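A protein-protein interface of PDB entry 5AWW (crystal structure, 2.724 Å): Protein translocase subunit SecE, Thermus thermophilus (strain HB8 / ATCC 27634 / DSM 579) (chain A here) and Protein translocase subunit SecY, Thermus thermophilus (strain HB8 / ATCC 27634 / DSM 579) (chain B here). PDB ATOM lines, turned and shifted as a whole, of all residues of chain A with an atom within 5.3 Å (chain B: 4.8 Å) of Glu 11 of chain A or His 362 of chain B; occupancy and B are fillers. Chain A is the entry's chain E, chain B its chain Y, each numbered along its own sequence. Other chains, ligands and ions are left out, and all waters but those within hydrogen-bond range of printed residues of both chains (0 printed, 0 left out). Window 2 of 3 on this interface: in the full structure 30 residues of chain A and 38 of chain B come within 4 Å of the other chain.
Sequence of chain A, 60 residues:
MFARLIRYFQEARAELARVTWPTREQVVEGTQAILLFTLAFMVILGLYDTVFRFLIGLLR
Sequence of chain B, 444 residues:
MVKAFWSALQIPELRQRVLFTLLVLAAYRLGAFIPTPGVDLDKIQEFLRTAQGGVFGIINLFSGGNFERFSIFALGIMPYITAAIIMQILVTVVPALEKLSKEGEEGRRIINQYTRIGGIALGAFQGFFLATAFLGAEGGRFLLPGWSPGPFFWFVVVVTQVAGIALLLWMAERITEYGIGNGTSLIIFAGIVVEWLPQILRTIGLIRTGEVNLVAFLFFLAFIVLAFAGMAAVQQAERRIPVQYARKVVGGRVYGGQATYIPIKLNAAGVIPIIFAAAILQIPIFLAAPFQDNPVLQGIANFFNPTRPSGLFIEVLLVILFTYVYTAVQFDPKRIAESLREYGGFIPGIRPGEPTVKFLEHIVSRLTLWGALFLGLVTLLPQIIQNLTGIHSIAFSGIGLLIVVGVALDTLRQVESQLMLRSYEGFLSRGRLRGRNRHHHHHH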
ATOM      1  N   ARG A   7      -8.586  -9.284 -26.895  1.00  0.00           N
ATOM      2  CA  ARG A   7      -9.139 -10.242 -25.944  1.00  0.00           C
ATOM      3  C   ARG A   7      -9.786  -9.493 -24.784  1.00  0.00           C
ATOM      4  O   ARG A   7     -10.881  -9.843 -24.326  1.00  0.00           O
ATOM      5  CB  ARG A   7      -8.050 -11.184 -25.427  1.00  0.00           C
ATOM      6  CG  ARG A   7      -8.537 -12.191 -24.401  1.00  0.00           C
ATOM      7  CD  ARG A   7      -7.369 -12.876 -23.712  1.00  0.00           C
ATOM      8  NE  ARG A   7      -6.536 -11.921 -22.985  1.00  0.00           N
ATOM      9  CZ  ARG A   7      -5.475 -12.254 -22.259  1.00  0.00           C
ATOM     10  NH1 ARG A   7      -5.110 -13.526 -22.160  1.00  0.00           N
ATOM     11  NH2 ARG A   7      -4.776 -11.317 -21.631  1.00  0.00           N
ATOM     12  N   TYR A   8      -9.089  -8.459 -24.320  1.00  0.00           N
ATOM     13  CA  TYR A   8      -9.584  -7.590 -23.259  1.00  0.00           C
ATOM     14  C   TYR A   8     -10.941  -7.000 -23.626  1.00  0.00           C
ATOM     15  O   TYR A   8     -11.823  -6.883 -22.778  1.00  0.00           O
ATOM     16  CB  TYR A   8      -8.576  -6.472 -22.973  1.00  0.00           C
ATOM     17  CG  TYR A   8      -9.046  -5.450 -21.960  1.00  0.00           C
ATOM     18  CD1 TYR A   8      -8.865  -5.660 -20.599  1.00  0.00           C
ATOM     19  CD2 TYR A   8      -9.658  -4.272 -22.366  1.00  0.00           C
ATOM     20  CE1 TYR A   8      -9.289  -4.726 -19.670  1.00  0.00           C
ATOM     21  CE2 TYR A   8     -10.088  -3.335 -21.445  1.00  0.00           C
ATOM     22  CZ  TYR A   8      -9.900  -3.567 -20.099  1.00  0.00           C
ATOM     23  OH  TYR A   8     -10.325  -2.635 -19.181  1.00  0.00           O
ATOM     24  N   PHE A   9     -11.098  -6.631 -24.894  1.00  0.00           N
ATOM     25  CA  PHE A   9     -12.354  -6.071 -25.379  1.00  0.00           C
ATOM     26  C   PHE A   9     -13.488  -7.084 -25.257  1.00  0.00           C
ATOM     27  O   PHE A   9     -14.596  -6.745 -24.843  1.00  0.00           O
ATOM     28  CB  PHE A   9     -12.209  -5.609 -26.830  1.00  0.00           C
ATOM     29  CG  PHE A   9     -13.446  -4.960 -27.387  1.00  0.00           C
ATOM     30  CD1 PHE A   9     -13.736  -3.634 -27.102  1.00  0.00           C
ATOM     31  CD2 PHE A   9     -14.314  -5.672 -28.199  1.00  0.00           C
ATOM     32  CE1 PHE A   9     -14.871  -3.033 -27.612  1.00  0.00           C
ATOM     33  CE2 PHE A   9     -15.452  -5.076 -28.713  1.00  0.00           C
ATOM     34  CZ  PHE A   9     -15.731  -3.755 -28.419  1.00  0.00           C
ATOM     35  N   GLN A  10     -13.198  -8.332 -25.615  1.00  0.00           N
ATOM     36  CA  GLN A  10     -14.193  -9.397 -25.554  1.00  0.00           C
ATOM     37  C   GLN A  10     -14.596  -9.697 -24.115  1.00  0.00           C
ATOM     38  O   GLN A  10     -15.781  -9.861 -23.815  1.00  0.00           O
ATOM     39  CB  GLN A  10     -13.659 -10.664 -26.224  1.00  0.00           C
ATOM     40  CG  GLN A  10     -13.302 -10.483 -27.687  1.00  0.00           C
ATOM     41  CD  GLN A  10     -12.642 -11.709 -28.279  1.00  0.00           C
ATOM     42  OE1 GLN A  10     -12.737 -12.807 -27.730  1.00  0.00           O
ATOM     43  NE2 GLN A  10     -11.960 -11.530 -29.405  1.00  0.00           N
ATOM     44  N   GLU A  11     -13.607  -9.767 -23.230  1.00  0.00           N
ATOM     45  CA  GLU A  11     -13.874 -10.041 -21.821  1.00  0.00           C
ATOM     46  C   GLU A  11     -14.672  -8.908 -21.177  1.00  0.00           C
ATOM     47  O   GLU A  11     -15.613  -9.150 -20.416  1.00  0.00           O
ATOM     48  CB  GLU A  11     -12.567 -10.263 -21.065  1.00  0.00           C
ATOM     49  CG  GLU A  11     -11.752 -11.432 -21.587  1.00  0.00           C
ATOM     50  CD  GLU A  11     -10.431 -11.583 -20.869  1.00  0.00           C
ATOM     51  OE1 GLU A  11     -10.173 -10.796 -19.935  1.00  0.00           O
ATOM     52  OE2 GLU A  11      -9.652 -12.486 -21.237  1.00  0.00           O
ATOM     53  N   ALA A  12     -14.293  -7.674 -21.492  1.00  0.00           N
ATOM     54  CA  ALA A  12     -15.002  -6.497 -21.006  1.00  0.00           C
ATOM     55  C   ALA A  12     -16.434  -6.479 -21.528  1.00  0.00           C
ATOM     56  O   ALA A  12     -17.352  -6.039 -20.839  1.00  0.00           O
ATOM     57  CB  ALA A  12     -14.272  -5.229 -21.416  1.00  0.00           C
ATOM     58  N   ARG A  13     -16.610  -6.959 -22.754  1.00  0.00           N
ATOM     59  CA  ARG A  13     -17.929  -7.056 -23.370  1.00  0.00           C
ATOM     60  C   ARG A  13     -18.780  -8.085 -22.630  1.00  0.00           C
ATOM     61  O   ARG A  13     -19.980  -7.879 -22.402  1.00  0.00           O
ATOM     62  CB  ARG A  13     -17.791  -7.426 -24.847  1.00  0.00           C
ATOM     63  CG  ARG A  13     -19.060  -7.291 -25.664  1.00  0.00           C
ATOM     64  CD  ARG A  13     -18.775  -7.611 -27.120  1.00  0.00           C
ATOM     65  NE  ARG A  13     -19.954  -7.466 -27.965  1.00  0.00           N
ATOM     66  CZ  ARG A  13     -19.960  -7.689 -29.275  1.00  0.00           C
ATOM     67  NH1 ARG A  13     -18.848  -8.068 -29.889  1.00  0.00           N
ATOM     68  NH2 ARG A  13     -21.077  -7.533 -29.971  1.00  0.00           N
ATOM     69  N   ALA A  14     -18.141  -9.189 -22.253  1.00  0.00           N
ATOM     70  CA  ALA A  14     -18.797 -10.230 -21.474  1.00  0.00           C
ATOM     71  C   ALA A  14     -19.232  -9.694 -20.114  1.00  0.00           C
ATOM     72  O   ALA A  14     -20.333  -9.988 -19.645  1.00  0.00           O
ATOM     73  CB  ALA A  14     -17.875 -11.426 -21.305  1.00  0.00           C
ATOM     74  N   GLU A  15     -18.368  -8.902 -19.487  1.00  0.00           N
ATOM     75  CA  GLU A  15     -18.701  -8.284 -18.207  1.00  0.00           C
ATOM     76  C   GLU A  15     -19.811  -7.249 -18.368  1.00  0.00           C
ATOM     77  O   GLU A  15     -20.603  -7.029 -17.452  1.00  0.00           O
ATOM     78  CB  GLU A  15     -17.466  -7.640 -17.577  1.00  0.00           C
ATOM     79  CG  GLU A  15     -16.470  -8.636 -17.003  1.00  0.00           C
ATOM     80  CD  GLU A  15     -17.012  -9.385 -15.798  1.00  0.00           C
ATOM     81  OE1 GLU A  15     -17.990  -8.908 -15.180  1.00  0.00           O
ATOM     82  OE2 GLU A  15     -16.456 -10.453 -15.467  1.00  0.00           O
ATOM     83  N   LEU A  16     -19.861  -6.616 -19.535  1.00  0.00           N
ATOM     84  CA  LEU A  16     -20.941  -5.690 -19.851  1.00  0.00           C
ATOM     85  C   LEU A  16     -22.255  -6.453 -19.938  1.00  0.00           C
ATOM     86  O   LEU A  16     -23.304  -5.952 -19.530  1.00  0.00           O
ATOM     87  CB  LEU A  16     -20.664  -4.949 -21.161  1.00  0.00           C
ATOM     88  CG  LEU A  16     -21.739  -3.963 -21.630  1.00  0.00           C
ATOM     89  CD1 LEU A  16     -21.931  -2.847 -20.614  1.00  0.00           C
ATOM     90  CD2 LEU A  16     -21.396  -3.395 -23.000  1.00  0.00           C
ATOM     91  N   VAL B 357      -8.588 -11.808  -4.862  1.00  0.00           N
ATOM     92  CA  VAL B 357      -8.189 -10.474  -5.292  1.00  0.00           C
ATOM     93  C   VAL B 357      -8.014 -10.431  -6.808  1.00  0.00           C
ATOM     94  O   VAL B 357      -8.346  -9.439  -7.449  1.00  0.00           O
ATOM     95  CB  VAL B 357      -6.880 -10.033  -4.607  1.00  0.00           C
ATOM     96  CG1 VAL B 357      -6.540  -8.598  -4.978  1.00  0.00           C
ATOM     97  CG2 VAL B 357      -7.001 -10.177  -3.098  1.00  0.00           C
ATOM     98  N   LYS B 358      -7.496 -11.517  -7.373  1.00  0.00           N
ATOM     99  CA  LYS B 358      -7.345 -11.650  -8.818  1.00  0.00           C
ATOM    100  C   LYS B 358      -8.705 -11.644  -9.509  1.00  0.00           C
ATOM    101  O   LYS B 358      -8.889 -10.980 -10.532  1.00  0.00           O
ATOM    102  CB  LYS B 358      -6.579 -12.934  -9.161  1.00  0.00           C
ATOM    103  CG  LYS B 358      -6.812 -13.459 -10.575  1.00  0.00           C
ATOM    104  CD  LYS B 358      -6.268 -12.515 -11.640  1.00  0.00           C
ATOM    105  CE  LYS B 358      -6.699 -12.955 -13.032  1.00  0.00           C
ATOM    106  NZ  LYS B 358      -6.279 -11.990 -14.085  1.00  0.00           N
ATOM    107  N   PHE B 359      -9.651 -12.389  -8.947  1.00  0.00           N
ATOM    108  CA  PHE B 359     -11.005 -12.452  -9.485  1.00  0.00           C
ATOM    109  C   PHE B 359     -11.651 -11.067  -9.492  1.00  0.00           C
ATOM    110  O   PHE B 359     -12.148 -10.596 -10.528  1.00  0.00           O
ATOM    111  CB  PHE B 359     -11.844 -13.439  -8.671  1.00  0.00           C
ATOM    112  CG  PHE B 359     -13.192 -13.733  -9.264  1.00  0.00           C
ATOM    113  CD1 PHE B 359     -13.303 -14.246 -10.545  1.00  0.00           C
ATOM    114  CD2 PHE B 359     -14.348 -13.518  -8.529  1.00  0.00           C
ATOM    115  CE1 PHE B 359     -14.543 -14.523 -11.091  1.00  0.00           C
ATOM    116  CE2 PHE B 359     -15.590 -13.795  -9.066  1.00  0.00           C
ATOM    117  CZ  PHE B 359     -15.688 -14.298 -10.348  1.00  0.00           C
ATOM    118  N   LEU B 360     -11.620 -10.415  -8.332  1.00  0.00           N
ATOM    119  CA  LEU B 360     -12.184  -9.077  -8.176  1.00  0.00           C
ATOM    120  C   LEU B 360     -11.538  -8.071  -9.124  1.00  0.00           C
ATOM    121  O   LEU B 360     -12.232  -7.325  -9.815  1.00  0.00           O
ATOM    122  CB  LEU B 360     -12.031  -8.599  -6.732  1.00  0.00           C
ATOM    123  CG  LEU B 360     -12.795  -9.388  -5.668  1.00  0.00           C
ATOM    124  CD1 LEU B 360     -12.533  -8.816  -4.284  1.00  0.00           C
ATOM    125  CD2 LEU B 360     -14.283  -9.396  -5.976  1.00  0.00           C
ATOM    126  N   GLU B 361     -10.209  -8.060  -9.152  1.00  0.00           N
ATOM    127  CA  GLU B 361      -9.457  -7.149 -10.008  1.00  0.00           C
ATOM    128  C   GLU B 361      -9.815  -7.361 -11.473  1.00  0.00           C
ATOM    129  O   GLU B 361      -9.979  -6.399 -12.221  1.00  0.00           O
ATOM    130  CB  GLU B 361      -7.950  -7.329  -9.795  1.00  0.00           C
ATOM    131  CG  GLU B 361      -7.074  -6.381 -10.607  1.00  0.00           C
ATOM    132  CD  GLU B 361      -6.723  -6.931 -11.978  1.00  0.00           C
ATOM    133  OE1 GLU B 361      -6.880  -8.153 -12.188  1.00  0.00           O
ATOM    134  OE2 GLU B 361      -6.293  -6.142 -12.846  1.00  0.00           O
ATOM    135  N   HIS B 362      -9.935  -8.623 -11.873  1.00  0.00           N
ATOM    136  CA  HIS B 362     -10.307  -8.963 -13.241  1.00  0.00           C
ATOM    137  C   HIS B 362     -11.678  -8.390 -13.584  1.00  0.00           C
ATOM    138  O   HIS B 362     -11.829  -7.654 -14.567  1.00  0.00           O
ATOM    139  CB  HIS B 362     -10.299 -10.480 -13.441  1.00  0.00           C
ATOM    140  CG  HIS B 362     -10.638 -10.911 -14.834  1.00  0.00           C
ATOM    141  ND1 HIS B 362     -11.936 -11.095 -15.263  1.00  0.00           N
ATOM    142  CD2 HIS B 362      -9.848 -11.204 -15.894  1.00  0.00           C
ATOM    143  CE1 HIS B 362     -11.931 -11.477 -16.527  1.00  0.00           C
ATOM    144  NE2 HIS B 362     -10.677 -11.552 -16.934  1.00  0.00           N
ATOM    145  N   ILE B 363     -12.671  -8.714 -12.757  1.00  0.00           N
ATOM    146  CA  ILE B 363     -14.033  -8.241 -12.992  1.00  0.00           C
ATOM    147  C   ILE B 363     -14.105  -6.713 -13.062  1.00  0.00           C
ATOM    148  O   ILE B 363     -14.692  -6.160 -13.992  1.00  0.00           O
ATOM    149  CB  ILE B 363     -15.001  -8.744 -11.904  1.00  0.00           C
ATOM    150  CG1 ILE B 363     -15.096 -10.270 -11.947  1.00  0.00           C
ATOM    151  CG2 ILE B 363     -16.380  -8.130 -12.090  1.00  0.00           C
ATOM    152  CD1 ILE B 363     -16.154 -10.842 -11.032  1.00  0.00           C
ATOM    153  N   VAL B 364     -13.492  -6.039 -12.093  1.00  0.00           N
ATOM    154  CA  VAL B 364     -13.513  -4.577 -12.035  1.00  0.00           C
ATOM    155  C   VAL B 364     -12.830  -3.937 -13.242  1.00  0.00           C
ATOM    156  O   VAL B 364     -13.385  -3.029 -13.878  1.00  0.00           O
ATOM    157  CB  VAL B 364     -12.837  -4.054 -10.750  1.00  0.00           C
ATOM    158  CG1 VAL B 364     -12.667  -2.543 -10.811  1.00  0.00           C
ATOM    159  CG2 VAL B 364     -13.643  -4.453  -9.525  1.00  0.00           C
ATOM    160  N   SER B 365     -11.627  -4.415 -13.550  1.00  0.00           N
ATOM    161  CA  SER B 365     -10.843  -3.878 -14.656  1.00  0.00           C
ATOM    162  C   SER B 365     -11.561  -4.068 -15.985  1.00  0.00           C
ATOM    163  O   SER B 365     -11.466  -3.221 -16.872  1.00  0.00           O
ATOM    164  CB  SER B 365      -9.463  -4.534 -14.711  1.00  0.00           C
ATOM    165  OG  SER B 365      -9.563  -5.912 -15.024  1.00  0.00           O
ATOM    166  N   ARG B 366     -12.282  -5.178 -16.123  1.00  0.00           N
ATOM    167  CA  ARG B 366     -13.053  -5.412 -17.341  1.00  0.00           C
ATOM    168  C   ARG B 366     -14.337  -4.582 -17.360  1.00  0.00           C
ATOM    169  O   ARG B 366     -14.851  -4.240 -18.423  1.00  0.00           O
ATOM    170  CB  ARG B 366     -13.395  -6.897 -17.495  1.00  0.00           C
ATOM    171  CG  ARG B 366     -12.196  -7.826 -17.640  1.00  0.00           C
ATOM    172  CD  ARG B 366     -11.336  -7.466 -18.838  1.00  0.00           C
ATOM    173  NE  ARG B 366     -10.228  -8.401 -19.021  1.00  0.00           N
ATOM    174  CZ  ARG B 366      -9.067  -8.324 -18.379  1.00  0.00           C
ATOM    175  NH1 ARG B 366      -8.855  -7.353 -17.500  1.00  0.00           N
ATOM    176  NH2 ARG B 366      -8.117  -9.220 -18.611  1.00  0.00           N
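A ring nitrogen (NE2) of His 362 of chain B sits at hydrogen-bond distance from the side-chain carboxylate of Glu 11 of chain A (3.1 Å).
O of Ser 365 of chain B is in hydrogen-bond range of OH of Tyr 8 of chain A (2.6 Å).
NE of Arg 366 of chain B lies within salt-bridge range of OE1 of Glu 11 of chain A (2.6 Å).
The backbone carbonyl oxygen (O) of Glu 361 of chain B lies within hydrogen-bond range of the side-chain hydroxyl (OG) of Ser 365 of chain B (2.9 Å).
The backbone carbonyl oxygen of His 362 of chain B is in hydrogen-bond range of the side-chain hydroxyl of Ser 365 of chain B (2.9 Å).
OG of Ser 365 of chain B sits at hydrogen-bond distance from NH1 of Arg 366 of chain B (3.0 Å).
NE of Arg 7 of chain A lies within salt-bridge range of OE2 of Glu 11 of chain A (3.6 Å).
Arg 366 of chain B touches Tyr 8 of chain A.
Ala 12 of chain A touches Arg 366 of chain B (CB to O, 3.2 Å).
CG2 of Ile 363 of chain B touches OE1 of Glu 15 of chain A, 3.6 Å away.
CG of Glu 15 of chain A touches CB of Arg 366 of chain B, 3.6 Å away.
Of the printed residues of chain B, Tyr 8 of chain A touches Ser 365 and Arg 366.
Printed residues of chain B within 4 Å of Glu 11 of chain A: His 362 and Arg 366.
His 362 of chain B touches just one residue of chain A: Glu 11 (3.1 Å).
Of the printed residues of chain A, Ile 363 of chain B touches Glu 15.
The nearest printed residue of chain B that does not touch Glu 11 of chain A is Ser 365 of chain B (7.0 Å).
Of the 10 printed residues of chain B, 4 touch a printed residue of chain A.
Along chain B the printed residues that touch a printed residue of chain A span positions 362 to 366.
Of the 10 printed residues of chain A, 4 touch a printed residue of chain B.
Hydrophobic or aromatic side chains of chain A within 4 Å of the printed part of chain B: Tyr 8 and Ala 12.
Among the printed residues, 7 pairs touch across the chains.
Among the printed residues, Asp or Glu carboxylates within 4 Å of a Lys or Arg side-chain nitrogen of the other chain: Glu 11 of chain A with Arg 366 of chain B (2.6 Å).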
